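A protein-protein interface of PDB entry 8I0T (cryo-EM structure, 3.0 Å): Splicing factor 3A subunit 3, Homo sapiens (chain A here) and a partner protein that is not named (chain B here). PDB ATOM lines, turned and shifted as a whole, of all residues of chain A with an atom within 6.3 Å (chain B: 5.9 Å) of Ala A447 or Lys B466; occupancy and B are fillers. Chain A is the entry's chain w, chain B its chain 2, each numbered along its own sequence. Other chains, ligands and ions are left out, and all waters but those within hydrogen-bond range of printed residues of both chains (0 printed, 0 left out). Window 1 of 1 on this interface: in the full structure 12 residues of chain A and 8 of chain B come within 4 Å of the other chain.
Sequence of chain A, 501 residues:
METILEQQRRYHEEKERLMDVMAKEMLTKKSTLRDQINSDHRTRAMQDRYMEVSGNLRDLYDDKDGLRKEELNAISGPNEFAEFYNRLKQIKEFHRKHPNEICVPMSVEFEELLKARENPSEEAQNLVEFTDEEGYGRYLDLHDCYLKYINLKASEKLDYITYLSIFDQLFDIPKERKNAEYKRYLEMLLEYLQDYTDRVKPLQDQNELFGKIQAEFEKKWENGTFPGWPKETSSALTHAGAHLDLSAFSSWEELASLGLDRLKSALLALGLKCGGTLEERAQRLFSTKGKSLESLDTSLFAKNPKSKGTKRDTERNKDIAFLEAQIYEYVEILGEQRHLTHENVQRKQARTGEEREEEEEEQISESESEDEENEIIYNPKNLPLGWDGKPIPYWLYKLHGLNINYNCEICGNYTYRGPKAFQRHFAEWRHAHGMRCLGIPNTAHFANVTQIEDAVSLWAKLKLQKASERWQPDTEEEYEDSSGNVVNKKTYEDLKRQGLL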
ATOM      1  N   PHE A 426     -23.109  10.172  -0.720  1.00  0.00           N
ATOM      2  CA  PHE A 426     -21.976  10.816  -0.071  1.00  0.00           C
ATOM      3  C   PHE A 426     -22.408  12.065   0.681  1.00  0.00           C
ATOM      4  O   PHE A 426     -21.752  12.463   1.646  1.00  0.00           O
ATOM      5  CB  PHE A 426     -20.900  11.136  -1.102  1.00  0.00           C
ATOM      6  CG  PHE A 426     -20.095   9.946  -1.507  1.00  0.00           C
ATOM      7  CD1 PHE A 426     -19.026   9.531  -0.751  1.00  0.00           C
ATOM      8  CD2 PHE A 426     -20.421   9.233  -2.639  1.00  0.00           C
ATOM      9  CE1 PHE A 426     -18.302   8.426  -1.104  1.00  0.00           C
ATOM     10  CE2 PHE A 426     -19.689   8.132  -3.008  1.00  0.00           C
ATOM     11  CZ  PHE A 426     -18.628   7.727  -2.240  1.00  0.00           C
ATOM     12  N   HIS A 431     -23.734   8.622   5.345  1.00  0.00           N
ATOM     13  CA  HIS A 431     -22.378   9.089   5.107  1.00  0.00           C
ATOM     14  C   HIS A 431     -22.038  10.277   5.997  1.00  0.00           C
ATOM     15  O   HIS A 431     -20.916  10.369   6.510  1.00  0.00           O
ATOM     16  CB  HIS A 431     -22.214   9.429   3.631  1.00  0.00           C
ATOM     17  CG  HIS A 431     -20.891   9.028   3.078  1.00  0.00           C
ATOM     18  ND1 HIS A 431     -20.454   7.721   3.071  1.00  0.00           N
ATOM     19  CD2 HIS A 431     -19.912   9.758   2.499  1.00  0.00           C
ATOM     20  CE1 HIS A 431     -19.252   7.668   2.527  1.00  0.00           C
ATOM     21  NE2 HIS A 431     -18.898   8.889   2.178  1.00  0.00           N
ATOM     22  N   ASN A 442     -17.979  16.426   6.909  1.00  0.00           N
ATOM     23  CA  ASN A 442     -18.504  15.999   5.616  1.00  0.00           C
ATOM     24  C   ASN A 442     -18.356  17.144   4.618  1.00  0.00           C
ATOM     25  O   ASN A 442     -19.327  17.672   4.070  1.00  0.00           O
ATOM     26  CB  ASN A 442     -19.960  15.567   5.744  1.00  0.00           C
ATOM     27  CG  ASN A 442     -20.360  14.544   4.702  1.00  0.00           C
ATOM     28  OD1 ASN A 442     -19.523  14.047   3.951  1.00  0.00           O
ATOM     29  ND2 ASN A 442     -21.647  14.237   4.640  1.00  0.00           N
ATOM     30  N   THR A 443     -17.111  17.535   4.378  1.00  0.00           N
ATOM     31  CA  THR A 443     -16.776  18.452   3.300  1.00  0.00           C
ATOM     32  C   THR A 443     -16.459  17.627   2.053  1.00  0.00           C
ATOM     33  O   THR A 443     -16.199  16.422   2.122  1.00  0.00           O
ATOM     34  CB  THR A 443     -15.619  19.385   3.702  1.00  0.00           C
ATOM     35  OG1 THR A 443     -14.367  18.699   3.602  1.00  0.00           O
ATOM     36  CG2 THR A 443     -15.796  19.888   5.128  1.00  0.00           C
ATOM     37  N   ALA A 444     -16.508  18.283   0.894  1.00  0.00           N
ATOM     38  CA  ALA A 444     -16.511  17.540  -0.361  1.00  0.00           C
ATOM     39  C   ALA A 444     -15.195  16.817  -0.583  1.00  0.00           C
ATOM     40  O   ALA A 444     -15.146  15.803  -1.288  1.00  0.00           O
ATOM     41  CB  ALA A 444     -16.807  18.477  -1.530  1.00  0.00           C
ATOM     42  N   HIS A 445     -14.126  17.306   0.043  1.00  0.00           N
ATOM     43  CA  HIS A 445     -12.777  16.940  -0.367  1.00  0.00           C
ATOM     44  C   HIS A 445     -12.541  15.442  -0.286  1.00  0.00           C
ATOM     45  O   HIS A 445     -11.655  14.920  -0.968  1.00  0.00           O
ATOM     46  CB  HIS A 445     -11.753  17.680   0.489  1.00  0.00           C
ATOM     47  CG  HIS A 445     -11.995  19.154   0.599  1.00  0.00           C
ATOM     48  ND1 HIS A 445     -11.058  20.020   1.117  1.00  0.00           N
ATOM     49  CD2 HIS A 445     -13.067  19.914   0.275  1.00  0.00           C
ATOM     50  CE1 HIS A 445     -11.538  21.248   1.103  1.00  0.00           C
ATOM     51  NE2 HIS A 445     -12.757  21.211   0.599  1.00  0.00           N
ATOM     52  N   PHE A 446     -13.324  14.738   0.528  1.00  0.00           N
ATOM     53  CA  PHE A 446     -13.170  13.309   0.747  1.00  0.00           C
ATOM     54  C   PHE A 446     -14.231  12.496   0.032  1.00  0.00           C
ATOM     55  O   PHE A 446     -14.077  11.277  -0.084  1.00  0.00           O
ATOM     56  CB  PHE A 446     -13.226  13.004   2.240  1.00  0.00           C
ATOM     57  CG  PHE A 446     -12.835  14.161   3.094  1.00  0.00           C
ATOM     58  CD1 PHE A 446     -11.506  14.515   3.235  1.00  0.00           C
ATOM     59  CD2 PHE A 446     -13.797  14.925   3.724  1.00  0.00           C
ATOM     60  CE1 PHE A 446     -11.145  15.586   4.009  1.00  0.00           C
ATOM     61  CE2 PHE A 446     -13.439  15.997   4.498  1.00  0.00           C
ATOM     62  CZ  PHE A 446     -12.114  16.330   4.639  1.00  0.00           C
ATOM     63  N   ALA A 447     -15.309  13.131  -0.418  1.00  0.00           N
ATOM     64  CA  ALA A 447     -16.347  12.420  -1.147  1.00  0.00           C
ATOM     65  C   ALA A 447     -15.730  11.550  -2.229  1.00  0.00           C
ATOM     66  O   ALA A 447     -14.864  11.993  -2.984  1.00  0.00           O
ATOM     67  CB  ALA A 447     -17.335  13.410  -1.757  1.00  0.00           C
ATOM     68  N   ASN A 448     -16.171  10.300  -2.279  1.00  0.00           N
ATOM     69  CA  ASN A 448     -15.695   9.184  -3.094  1.00  0.00           C
ATOM     70  C   ASN A 448     -14.433   8.552  -2.531  1.00  0.00           C
ATOM     71  O   ASN A 448     -13.933   7.595  -3.129  1.00  0.00           O
ATOM     72  CB  ASN A 448     -15.459   9.537  -4.567  1.00  0.00           C
ATOM     73  CG  ASN A 448     -16.352   8.749  -5.492  1.00  0.00           C
ATOM     74  OD1 ASN A 448     -17.112   7.897  -5.046  1.00  0.00           O
ATOM     75  ND2 ASN A 448     -16.279   9.034  -6.782  1.00  0.00           N
ATOM     76  N   VAL A 449     -13.907   9.024  -1.415  1.00  0.00           N
ATOM     77  CA  VAL A 449     -12.956   8.231  -0.648  1.00  0.00           C
ATOM     78  C   VAL A 449     -13.719   7.486   0.433  1.00  0.00           C
ATOM     79  O   VAL A 449     -14.194   8.092   1.403  1.00  0.00           O
ATOM     80  CB  VAL A 449     -11.843   9.103  -0.047  1.00  0.00           C
ATOM     81  CG1 VAL A 449     -10.806   8.215   0.573  1.00  0.00           C
ATOM     82  CG2 VAL A 449     -11.186   9.921  -1.124  1.00  0.00           C
ATOM     83  N   THR A 450     -13.821   6.169   0.274  1.00  0.00           N
ATOM     84  CA  THR A 450     -14.693   5.333   1.088  1.00  0.00           C
ATOM     85  C   THR A 450     -13.971   4.542   2.169  1.00  0.00           C
ATOM     86  O   THR A 450     -14.610   4.124   3.132  1.00  0.00           O
ATOM     87  CB  THR A 450     -15.470   4.362   0.186  1.00  0.00           C
ATOM     88  OG1 THR A 450     -14.548   3.551  -0.553  1.00  0.00           O
ATOM     89  CG2 THR A 450     -16.346   5.130  -0.793  1.00  0.00           C
ATOM     90  N   LEU A 458      -5.666  11.395   4.065  1.00  0.00           N
ATOM     91  CA  LEU A 458      -6.095  12.531   3.261  1.00  0.00           C
ATOM     92  C   LEU A 458      -6.351  13.745   4.134  1.00  0.00           C
ATOM     93  O   LEU A 458      -5.684  14.777   3.988  1.00  0.00           O
ATOM     94  CB  LEU A 458      -7.366  12.165   2.495  1.00  0.00           C
ATOM     95  CG  LEU A 458      -7.643  12.706   1.095  1.00  0.00           C
ATOM     96  CD1 LEU A 458      -8.014  11.574   0.175  1.00  0.00           C
ATOM     97  CD2 LEU A 458      -8.761  13.726   1.147  1.00  0.00           C
ATOM     98  N   LYS A 461      -3.110  15.299   5.598  1.00  0.00           N
ATOM     99  CA  LYS A 461      -2.395  16.292   4.804  1.00  0.00           C
ATOM    100  C   LYS A 461      -3.231  17.550   4.609  1.00  0.00           C
ATOM    101  O   LYS A 461      -2.686  18.659   4.565  1.00  0.00           O
ATOM    102  CB  LYS A 461      -1.967  15.715   3.453  1.00  0.00           C
ATOM    103  CG  LYS A 461      -3.085  15.512   2.469  1.00  0.00           C
ATOM    104  CD  LYS A 461      -2.541  15.164   1.105  1.00  0.00           C
ATOM    105  CE  LYS A 461      -2.534  16.392   0.223  1.00  0.00           C
ATOM    106  NZ  LYS A 461      -3.035  16.112  -1.147  1.00  0.00           N
ATOM    107  N   THR B 461      -6.384   5.043  -7.586  1.00  0.00           N
ATOM    108  CA  THR B 461      -7.529   5.182  -6.713  1.00  0.00           C
ATOM    109  C   THR B 461      -7.947   6.640  -6.623  1.00  0.00           C
ATOM    110  O   THR B 461      -7.135   7.552  -6.758  1.00  0.00           O
ATOM    111  CB  THR B 461      -7.202   4.696  -5.306  1.00  0.00           C
ATOM    112  OG1 THR B 461      -6.770   5.812  -4.526  1.00  0.00           O
ATOM    113  CG2 THR B 461      -6.074   3.694  -5.358  1.00  0.00           C
ATOM    114  N   VAL B 462      -9.236   6.855  -6.374  1.00  0.00           N
ATOM    115  CA  VAL B 462      -9.678   8.222  -6.167  1.00  0.00           C
ATOM    116  C   VAL B 462      -8.992   8.802  -4.943  1.00  0.00           C
ATOM    117  O   VAL B 462      -8.705  10.004  -4.891  1.00  0.00           O
ATOM    118  CB  VAL B 462     -11.207   8.274  -6.065  1.00  0.00           C
ATOM    119  CG1 VAL B 462     -11.681   9.697  -6.075  1.00  0.00           C
ATOM    120  CG2 VAL B 462     -11.814   7.517  -7.215  1.00  0.00           C
ATOM    121  N   ALA B 463      -8.640   7.959  -3.976  1.00  0.00           N
ATOM    122  CA  ALA B 463      -7.843   8.456  -2.864  1.00  0.00           C
ATOM    123  C   ALA B 463      -6.400   8.704  -3.275  1.00  0.00           C
ATOM    124  O   ALA B 463      -5.786   9.671  -2.807  1.00  0.00           O
ATOM    125  CB  ALA B 463      -7.892   7.481  -1.696  1.00  0.00           C
ATOM    126  N   GLU B 464      -5.851   7.842  -4.132  1.00  0.00           N
ATOM    127  CA  GLU B 464      -4.564   8.116  -4.752  1.00  0.00           C
ATOM    128  C   GLU B 464      -4.534   9.539  -5.284  1.00  0.00           C
ATOM    129  O   GLU B 464      -3.671  10.350  -4.922  1.00  0.00           O
ATOM    130  CB  GLU B 464      -4.313   7.113  -5.878  1.00  0.00           C
ATOM    131  CG  GLU B 464      -2.884   6.963  -6.295  1.00  0.00           C
ATOM    132  CD  GLU B 464      -2.163   5.888  -5.519  1.00  0.00           C
ATOM    133  OE1 GLU B 464      -2.168   5.942  -4.277  1.00  0.00           O
ATOM    134  OE2 GLU B 464      -1.582   4.985  -6.152  1.00  0.00           O
ATOM    135  N   LEU B 465      -5.521   9.868  -6.110  1.00  0.00           N
ATOM    136  CA  LEU B 465      -5.602  11.205  -6.664  1.00  0.00           C
ATOM    137  C   LEU B 465      -5.693  12.238  -5.559  1.00  0.00           C
ATOM    138  O   LEU B 465      -4.750  13.000  -5.333  1.00  0.00           O
ATOM    139  CB  LEU B 465      -6.799  11.311  -7.599  1.00  0.00           C
ATOM    140  CG  LEU B 465      -6.507  11.906  -8.972  1.00  0.00           C
ATOM    141  CD1 LEU B 465      -5.025  12.192  -9.085  1.00  0.00           C
ATOM    142  CD2 LEU B 465      -6.965  10.967 -10.084  1.00  0.00           C
ATOM    143  N   LYS B 466      -6.789  12.221  -4.794  1.00  0.00           N
ATOM    144  CA  LYS B 466      -7.038  13.317  -3.868  1.00  0.00           C
ATOM    145  C   LYS B 466      -5.858  13.577  -2.942  1.00  0.00           C
ATOM    146  O   LYS B 466      -5.595  14.733  -2.590  1.00  0.00           O
ATOM    147  CB  LYS B 466      -8.301  13.053  -3.061  1.00  0.00           C
ATOM    148  CG  LYS B 466      -9.497  12.796  -3.932  1.00  0.00           C
ATOM    149  CD  LYS B 466     -10.778  12.746  -3.141  1.00  0.00           C
ATOM    150  CE  LYS B 466     -11.958  12.433  -4.036  1.00  0.00           C
ATOM    151  NZ  LYS B 466     -13.178  13.213  -3.701  1.00  0.00           N
ATOM    152  N   GLN B 467      -5.101  12.540  -2.577  1.00  0.00           N
ATOM    153  CA  GLN B 467      -3.937  12.785  -1.736  1.00  0.00           C
ATOM    154  C   GLN B 467      -2.777  13.359  -2.543  1.00  0.00           C
ATOM    155  O   GLN B 467      -2.085  14.272  -2.081  1.00  0.00           O
ATOM    156  CB  GLN B 467      -3.516  11.503  -1.011  1.00  0.00           C
ATOM    157  CG  GLN B 467      -2.627  11.776   0.190  1.00  0.00           C
ATOM    158  CD  GLN B 467      -1.782  10.590   0.590  1.00  0.00           C
ATOM    159  OE1 GLN B 467      -2.289   9.594   1.105  1.00  0.00           O
ATOM    160  NE2 GLN B 467      -0.480  10.695   0.366  1.00  0.00           N
ATOM    161  N   LEU B 468      -2.532  12.823  -3.744  1.00  0.00           N
ATOM    162  CA  LEU B 468      -1.494  13.395  -4.598  1.00  0.00           C
ATOM    163  C   LEU B 468      -1.727  14.886  -4.826  1.00  0.00           C
ATOM    164  O   LEU B 468      -0.872  15.723  -4.512  1.00  0.00           O
ATOM    165  CB  LEU B 468      -1.456  12.666  -5.944  1.00  0.00           C
ATOM    166  CG  LEU B 468      -0.564  11.457  -6.209  1.00  0.00           C
ATOM    167  CD1 LEU B 468      -1.180  10.541  -7.251  1.00  0.00           C
ATOM    168  CD2 LEU B 468       0.783  11.941  -6.680  1.00  0.00           C
ATOM    169  N   VAL B 469      -2.913  15.222  -5.336  1.00  0.00           N
ATOM    170  CA  VAL B 469      -3.190  16.524  -5.917  1.00  0.00           C
ATOM    171  C   VAL B 469      -2.969  17.641  -4.899  1.00  0.00           C
ATOM    172  O   VAL B 469      -3.029  17.437  -3.680  1.00  0.00           O
ATOM    173  CB  VAL B 469      -4.632  16.517  -6.448  1.00  0.00           C
ATOM    174  CG1 VAL B 469      -5.045  17.859  -6.977  1.00  0.00           C
ATOM    175  CG2 VAL B 469      -4.770  15.475  -7.514  1.00  0.00           C
ATOM    176  N   ALA B 470      -2.697  18.841  -5.416  1.00  0.00           N
ATOM    177  CA  ALA B 470      -2.548  20.011  -4.563  1.00  0.00           C
ATOM    178  C   ALA B 470      -3.878  20.694  -4.278  1.00  0.00           C
ATOM    179  O   ALA B 470      -3.997  21.395  -3.269  1.00  0.00           O
ATOM    180  CB  ALA B 470      -1.577  20.997  -5.197  1.00  0.00           C
ATOM    181  N   PRO B 472      -7.794  19.543  -3.887  1.00  0.00           N
ATOM    182  CA  PRO B 472      -8.547  18.283  -3.915  1.00  0.00           C
ATOM    183  C   PRO B 472     -10.032  18.455  -4.162  1.00  0.00           C
ATOM    184  O   PRO B 472     -10.770  17.472  -4.235  1.00  0.00           O
ATOM    185  CB  PRO B 472      -8.287  17.714  -2.521  1.00  0.00           C
ATOM    186  CG  PRO B 472      -8.192  18.929  -1.669  1.00  0.00           C
ATOM    187  CD  PRO B 472      -7.628  20.045  -2.515  1.00  0.00           C
ATOM    188  N   VAL B 475     -11.433  16.694  -7.694  1.00  0.00           N
ATOM    189  CA  VAL B 475     -11.421  15.286  -8.052  1.00  0.00           C
ATOM    190  C   VAL B 475     -12.834  14.725  -8.015  1.00  0.00           C
ATOM    191  O   VAL B 475     -13.575  14.922  -7.045  1.00  0.00           O
ATOM    192  CB  VAL B 475     -10.463  14.519  -7.137  1.00  0.00           C
ATOM    193  CG1 VAL B 475      -9.550  13.693  -7.964  1.00  0.00           C
ATOM    194  CG2 VAL B 475      -9.629  15.487  -6.336  1.00  0.00           C
ATOM    195  N   GLU B 476     -13.240  14.101  -9.116  1.00  0.00           N
ATOM    196  CA  GLU B 476     -14.581  13.595  -9.336  1.00  0.00           C
ATOM    197  C   GLU B 476     -14.516  12.104  -9.625  1.00  0.00           C
ATOM    198  O   GLU B 476     -13.466  11.470  -9.494  1.00  0.00           O
ATOM    199  CB  GLU B 476     -15.253  14.369 -10.468  1.00  0.00           C
ATOM    200  CG  GLU B 476     -16.744  14.268 -10.516  1.00  0.00           C
ATOM    201  CD  GLU B 476     -17.256  14.374 -11.922  1.00  0.00           C
ATOM    202  OE1 GLU B 476     -17.414  15.511 -12.404  1.00  0.00           O
ATOM    203  OE2 GLU B 476     -17.462  13.321 -12.558  1.00  0.00           O
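Among the printed residues, merely in contact across the chains: His A445 with Lys B466 (3.2 Å), Val A449 with Lys B466 (3.5 Å), Leu A458 with Lys B466 (3.6 Å), Val A449 with Ala B463 (3.8 Å) and Phe A446 with Lys B466 (3.9 Å).
Of the 13 printed residues of chain B, 4 touch a printed residue of chain A. Of the 13 printed residues of chain A, 6 touch a printed residue of chain B.
Ala A447 touches just one residue of chain B: Lys B466 (2.2 Å). Lys B466 touches just these residues of chain A: His A445 (3.2 Å), Phe A446 (3.9 Å), Ala A447 (2.2 Å), Val A449 (3.5 Å), Leu A458 (3.6 Å) and Lys A461 (3.2 Å). Of the printed residues of chain B, Phe A446 touches Lys B466 (3.9 Å). Of the printed residues of chain B, Val A449 touches Ala B463 (3.8 Å) and Lys B466 (3.5 Å). Printed residues of chain B within 4 Å of Leu A458: Lys B466 (3.6 Å). Printed residues of chain A within 4 Å of Val B469: Lys A461. Val B462 touches none of the printed residues of chain A. Thr A450 touches none of the printed residues of chain B. The nearest residue of chain A that does not touch Lys B466 is Ala A444 (4.1 Å).
The side-chain amino group of Lys A461 lies within hydrogen-bond range of the backbone carbonyl oxygen of Lys B466. O of Val B469 is in hydrogen-bond range of NZ of Lys A461 (2.9 Å). The backbone carbonyl oxygen (O) of Ala A447 lies close to the side-chain amino group (NZ) of Lys B466 (2.2 Å). O of Gln B467 sits close to NZ of Lys A461.
The side-chain hydroxyl (OG1) of Thr B461 lies within hydrogen-bond range of the backbone NH (N) of Ala B463.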
